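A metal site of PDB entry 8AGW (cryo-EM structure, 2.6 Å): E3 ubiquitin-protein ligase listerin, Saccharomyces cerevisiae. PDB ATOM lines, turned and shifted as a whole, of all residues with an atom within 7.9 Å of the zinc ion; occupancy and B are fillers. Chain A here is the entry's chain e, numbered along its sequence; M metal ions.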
ATOM      1  N   GLU A1507      32.864  -5.367 -20.537  1.00  0.00           N
ATOM      2  CA  GLU A1507      31.852  -5.733 -19.558  1.00  0.00           C
ATOM      3  C   GLU A1507      30.473  -5.769 -20.192  1.00  0.00           C
ATOM      4  O   GLU A1507      30.198  -5.019 -21.120  1.00  0.00           O
ATOM      5  CB  GLU A1507      31.850  -4.736 -18.404  1.00  0.00           C
ATOM      6  CG  GLU A1507      33.168  -4.673 -17.655  1.00  0.00           C
ATOM      7  CD  GLU A1507      33.138  -3.688 -16.510  1.00  0.00           C
ATOM      8  OE1 GLU A1507      32.358  -2.732 -16.580  1.00  0.00           O
ATOM      9  OE2 GLU A1507      33.911  -3.872 -15.538  1.00  0.00           O
ATOM     10  N   CYS A1508      29.601  -6.634 -19.690  1.00  0.00           N
ATOM     11  CA  CYS A1508      28.234  -6.689 -20.199  1.00  0.00           C
ATOM     12  C   CYS A1508      27.539  -5.383 -19.913  1.00  0.00           C
ATOM     13  O   CYS A1508      27.648  -4.852 -18.829  1.00  0.00           O
ATOM     14  CB  CYS A1508      27.499  -7.849 -19.542  1.00  0.00           C
ATOM     15  SG  CYS A1508      25.705  -7.746 -19.537  1.00  0.00           S
ATOM     16  N   ALA A1509      26.807  -4.857 -20.896  1.00  0.00           N
ATOM     17  CA  ALA A1509      26.169  -3.559 -20.713  1.00  0.00           C
ATOM     18  C   ALA A1509      25.102  -3.531 -19.622  1.00  0.00           C
ATOM     19  O   ALA A1509      25.032  -2.582 -18.848  1.00  0.00           O
ATOM     20  CB  ALA A1509      25.586  -3.075 -22.034  1.00  0.00           C
ATOM     21  N   ILE A1510      24.267  -4.556 -19.559  1.00  0.00           N
ATOM     22  CA  ILE A1510      23.190  -4.584 -18.575  1.00  0.00           C
ATOM     23  C   ILE A1510      23.693  -4.616 -17.138  1.00  0.00           C
ATOM     24  O   ILE A1510      23.197  -3.877 -16.294  1.00  0.00           O
ATOM     25  CB  ILE A1510      22.238  -5.765 -18.829  1.00  0.00           C
ATOM     26  CG1 ILE A1510      21.771  -5.756 -20.283  1.00  0.00           C
ATOM     27  CG2 ILE A1510      21.043  -5.726 -17.892  1.00  0.00           C
ATOM     28  CD1 ILE A1510      20.732  -6.805 -20.596  1.00  0.00           C
ATOM     29  N   CYS A1511      24.700  -5.440 -16.854  1.00  0.00           N
ATOM     30  CA  CYS A1511      25.172  -5.569 -15.473  1.00  0.00           C
ATOM     31  C   CYS A1511      26.548  -4.979 -15.187  1.00  0.00           C
ATOM     32  O   CYS A1511      27.014  -5.049 -14.047  1.00  0.00           O
ATOM     33  CB  CYS A1511      25.130  -7.028 -15.032  1.00  0.00           C
ATOM     34  SG  CYS A1511      26.226  -8.130 -15.948  1.00  0.00           S
ATOM     35  N   TYR A1512      27.216  -4.420 -16.200  1.00  0.00           N
ATOM     36  CA  TYR A1512      28.521  -3.781 -16.016  1.00  0.00           C
ATOM     37  C   TYR A1512      29.572  -4.696 -15.384  1.00  0.00           C
ATOM     38  O   TYR A1512      30.371  -4.253 -14.561  1.00  0.00           O
ATOM     39  CB  TYR A1512      28.397  -2.460 -15.248  1.00  0.00           C
ATOM     40  CG  TYR A1512      29.357  -1.399 -15.704  1.00  0.00           C
ATOM     41  CD1 TYR A1512      29.378  -0.972 -17.029  1.00  0.00           C
ATOM     42  CD2 TYR A1512      30.246  -0.813 -14.823  1.00  0.00           C
ATOM     43  CE1 TYR A1512      30.264   0.004 -17.455  1.00  0.00           C
ATOM     44  CE2 TYR A1512      31.139   0.162 -15.237  1.00  0.00           C
ATOM     45  CZ  TYR A1512      31.138   0.565 -16.551  1.00  0.00           C
ATOM     46  OH  TYR A1512      32.012   1.539 -16.970  1.00  0.00           O
ATOM     47  N   SER A1513      29.552  -5.974 -15.749  1.00  0.00           N
ATOM     48  CA  SER A1513      30.552  -6.906 -15.237  1.00  0.00           C
ATOM     49  C   SER A1513      30.993  -7.842 -16.350  1.00  0.00           C
ATOM     50  O   SER A1513      30.180  -8.246 -17.169  1.00  0.00           O
ATOM     51  CB  SER A1513      29.980  -7.721 -14.082  1.00  0.00           C
ATOM     52  OG  SER A1513      28.840  -8.449 -14.494  1.00  0.00           O
ATOM     53  N   ILE A1514      32.274  -8.167 -16.390  1.00  0.00           N
ATOM     54  CA  ILE A1514      32.760  -9.129 -17.382  1.00  0.00           C
ATOM     55  C   ILE A1514      32.183 -10.512 -17.136  1.00  0.00           C
ATOM     56  O   ILE A1514      31.832 -11.226 -18.070  1.00  0.00           O
ATOM     57  CB  ILE A1514      34.287  -9.179 -17.450  1.00  0.00           C
ATOM     58  CG1 ILE A1514      34.881  -7.812 -17.132  1.00  0.00           C
ATOM     59  CG2 ILE A1514      34.730  -9.625 -18.827  1.00  0.00           C
ATOM     60  CD1 ILE A1514      36.379  -7.726 -17.369  1.00  0.00           C
ATOM     61  N   LEU A1515      32.085 -10.917 -15.877  1.00  0.00           N
ATOM     62  CA  LEU A1515      31.600 -12.251 -15.559  1.00  0.00           C
ATOM     63  C   LEU A1515      30.214 -12.203 -14.936  1.00  0.00           C
ATOM     64  O   LEU A1515      29.989 -11.463 -13.976  1.00  0.00           O
ATOM     65  CB  LEU A1515      32.575 -12.977 -14.628  1.00  0.00           C
ATOM     66  CG  LEU A1515      33.928 -13.357 -15.236  1.00  0.00           C
ATOM     67  CD1 LEU A1515      34.875 -13.874 -14.169  1.00  0.00           C
ATOM     68  CD2 LEU A1515      33.742 -14.383 -16.335  1.00  0.00           C
ATOM     69  N   HIS A1516      29.291 -12.992 -15.455  1.00  0.00           N
ATOM     70  CA  HIS A1516      27.950 -13.040 -14.903  1.00  0.00           C
ATOM     71  C   HIS A1516      28.082 -13.575 -13.499  1.00  0.00           C
ATOM     72  O   HIS A1516      28.794 -14.532 -13.278  1.00  0.00           O
ATOM     73  CB  HIS A1516      27.071 -13.970 -15.729  1.00  0.00           C
ATOM     74  CG  HIS A1516      25.600 -13.785 -15.509  1.00  0.00           C
ATOM     75  ND1 HIS A1516      24.906 -14.464 -14.524  1.00  0.00           N
ATOM     76  CD2 HIS A1516      24.693 -13.007 -16.142  1.00  0.00           C
ATOM     77  CE1 HIS A1516      23.634 -14.104 -14.569  1.00  0.00           C
ATOM     78  NE2 HIS A1516      23.484 -13.222 -15.537  1.00  0.00           N
ATOM     79  N   ALA A1517      27.429 -12.943 -12.534  1.00  0.00           N
ATOM     80  CA  ALA A1517      27.635 -13.385 -11.158  1.00  0.00           C
ATOM     81  C   ALA A1517      27.140 -14.806 -10.941  1.00  0.00           C
ATOM     82  O   ALA A1517      27.840 -15.611 -10.340  1.00  0.00           O
ATOM     83  CB  ALA A1517      26.940 -12.431 -10.196  1.00  0.00           C
ATOM     84  N   LYS A1521      30.351 -16.346 -16.450  1.00  0.00           N
ATOM     85  CA  LYS A1521      30.656 -16.412 -17.873  1.00  0.00           C
ATOM     86  C   LYS A1521      30.898 -15.067 -18.549  1.00  0.00           C
ATOM     87  O   LYS A1521      30.328 -14.063 -18.143  1.00  0.00           O
ATOM     88  CB  LYS A1521      29.537 -17.168 -18.609  1.00  0.00           C
ATOM     89  CG  LYS A1521      29.941 -17.703 -19.969  1.00  0.00           C
ATOM     90  CD  LYS A1521      28.728 -18.043 -20.818  1.00  0.00           C
ATOM     91  CE  LYS A1521      29.135 -18.426 -22.233  1.00  0.00           C
ATOM     92  NZ  LYS A1521      27.953 -18.679 -23.101  1.00  0.00           N
ATOM     93  N   PRO A1523      30.740 -12.155 -21.535  1.00  0.00           N
ATOM     94  CA  PRO A1523      29.519 -11.784 -22.255  1.00  0.00           C
ATOM     95  C   PRO A1523      29.607 -12.142 -23.720  1.00  0.00           C
ATOM     96  O   PRO A1523      30.113 -11.350 -24.519  1.00  0.00           O
ATOM     97  CB  PRO A1523      29.471 -10.256 -22.099  1.00  0.00           C
ATOM     98  CG  PRO A1523      30.497  -9.901 -21.083  1.00  0.00           C
ATOM     99  CD  PRO A1523      31.530 -10.968 -21.173  1.00  0.00           C
ATOM    100  N   LYS A1533      28.556  -5.627 -25.375  1.00  0.00           N
ATOM    101  CA  LYS A1533      28.435  -7.058 -25.166  1.00  0.00           C
ATOM    102  C   LYS A1533      27.503  -7.370 -24.024  1.00  0.00           C
ATOM    103  O   LYS A1533      27.602  -6.775 -22.962  1.00  0.00           O
ATOM    104  CB  LYS A1533      29.811  -7.654 -24.848  1.00  0.00           C
ATOM    105  CG  LYS A1533      30.832  -7.530 -25.963  1.00  0.00           C
ATOM    106  CD  LYS A1533      32.162  -8.149 -25.535  1.00  0.00           C
ATOM    107  CE  LYS A1533      33.223  -7.987 -26.612  1.00  0.00           C
ATOM    108  NZ  LYS A1533      34.572  -8.380 -26.117  1.00  0.00           N
ATOM    109  N   PHE A1534      26.586  -8.309 -24.235  1.00  0.00           N
ATOM    110  CA  PHE A1534      25.602  -8.648 -23.214  1.00  0.00           C
ATOM    111  C   PHE A1534      25.732 -10.095 -22.803  1.00  0.00           C
ATOM    112  O   PHE A1534      25.968 -10.954 -23.646  1.00  0.00           O
ATOM    113  CB  PHE A1534      24.180  -8.441 -23.739  1.00  0.00           C
ATOM    114  CG  PHE A1534      23.935  -7.081 -24.329  1.00  0.00           C
ATOM    115  CD1 PHE A1534      23.552  -6.027 -23.526  1.00  0.00           C
ATOM    116  CD2 PHE A1534      24.052  -6.871 -25.693  1.00  0.00           C
ATOM    117  CE1 PHE A1534      23.309  -4.778 -24.052  1.00  0.00           C
ATOM    118  CE2 PHE A1534      23.811  -5.620 -26.229  1.00  0.00           C
ATOM    119  CZ  PHE A1534      23.437  -4.578 -25.415  1.00  0.00           C
ATOM    120  N   HIS A1535      25.599 -10.384 -21.520  1.00  0.00           N
ATOM    121  CA  HIS A1535      25.599 -11.775 -21.098  1.00  0.00           C
ATOM    122  C   HIS A1535      24.330 -12.344 -21.699  1.00  0.00           C
ATOM    123  O   HIS A1535      23.319 -11.647 -21.767  1.00  0.00           O
ATOM    124  CB  HIS A1535      25.506 -11.933 -19.594  1.00  0.00           C
ATOM    125  CG  HIS A1535      26.712 -11.445 -18.845  1.00  0.00           C
ATOM    126  ND1 HIS A1535      26.634 -10.467 -17.879  1.00  0.00           N
ATOM    127  CD2 HIS A1535      28.014 -11.804 -18.918  1.00  0.00           C
ATOM    128  CE1 HIS A1535      27.842 -10.241 -17.397  1.00  0.00           C
ATOM    129  NE2 HIS A1535      28.698 -11.040 -18.011  1.00  0.00           N
ATOM    130  N   GLY A1536      24.359 -13.601 -22.101  1.00  0.00           N
ATOM    131  CA  GLY A1536      23.194 -14.173 -22.742  1.00  0.00           C
ATOM    132  C   GLY A1536      22.006 -14.172 -21.821  1.00  0.00           C
ATOM    133  O   GLY A1536      20.910 -13.824 -22.244  1.00  0.00           O
ATOM    134  N   ALA A1537      22.214 -14.523 -20.563  1.00  0.00           N
ATOM    135  CA  ALA A1537      21.123 -14.567 -19.607  1.00  0.00           C
ATOM    136  C   ALA A1537      20.489 -13.195 -19.378  1.00  0.00           C
ATOM    137  O   ALA A1537      19.267 -13.064 -19.359  1.00  0.00           O
ATOM    138  CB  ALA A1537      21.599 -15.144 -18.286  1.00  0.00           C
ATOM    139  N   CYS A1538      21.325 -12.160 -19.241  1.00  0.00           N
ATOM    140  CA  CYS A1538      20.806 -10.820 -19.053  1.00  0.00           C
ATOM    141  C   CYS A1538      20.003 -10.377 -20.267  1.00  0.00           C
ATOM    142  O   CYS A1538      18.929  -9.800 -20.131  1.00  0.00           O
ATOM    143  CB  CYS A1538      21.940  -9.831 -18.813  1.00  0.00           C
ATOM    144  SG  CYS A1538      22.976 -10.133 -17.373  1.00  0.00           S
ATOM    145  N   LEU A1539      20.521 -10.662 -21.450  1.00  0.00           N
ATOM    146  CA  LEU A1539      19.846 -10.255 -22.671  1.00  0.00           C
ATOM    147  C   LEU A1539      18.502 -10.936 -22.810  1.00  0.00           C
ATOM    148  O   LEU A1539      17.515 -10.303 -23.165  1.00  0.00           O
ATOM    149  CB  LEU A1539      20.706 -10.581 -23.886  1.00  0.00           C
ATOM    150  CG  LEU A1539      20.296  -9.937 -25.199  1.00  0.00           C
ATOM    151  CD1 LEU A1539      20.337  -8.426 -25.068  1.00  0.00           C
ATOM    152  CD2 LEU A1539      21.204 -10.404 -26.324  1.00  0.00           C
HETATM  153 ZN    ZN M   1      25.039  -9.071 -17.736  1.00  0.00          ZN
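SG of Cys 1508 sits close to N of Ile 1510 (3.5 Å). A ring nitrogen (NE2) of His 1535 is in hydrogen-bond range of the backbone carbonyl oxygen of Ile 1514 (3.1 Å). A ring nitrogen (NE2) of His 1535 is in hydrogen-bond range of the backbone NH of His 1516 (3.3 Å). The side-chain sulfur (SG) of Cys 1538 sits close to a ring nitrogen (NE2) of His 1516. The backbone carbonyl oxygen (O) of Ser 1513 sits close to a ring nitrogen (NE2) of His 1535. The side-chain hydroxyl (OG) of Ser 1513 sits close to the side-chain sulfur (SG) of Cys 1511, at 3.0 Å. The backbone carbonyl oxygen (O) of Lys 1521 lies close to a ring nitrogen (NE2) of His 1535 (3.4 Å). N of Cys 1508 lies within hydrogen-bond range of O of Ser 1513 (3.0 Å).
Within 4 Å of the zinc ion: Cys 1508, Cys 1511, His 1535 and Cys 1538. The nearest printed residue that does not touch the zinc ion is His 1516 (4.3 Å).
The zinc ion is bound by ND1 of His 1535 (2.1 Å), SG of Cys 1508 (2.3 Å), SG of Cys 1511 (2.3 Å) and SG of Cys 1538 (2.3 Å). The zinc ion has four donor atoms within binding distance.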
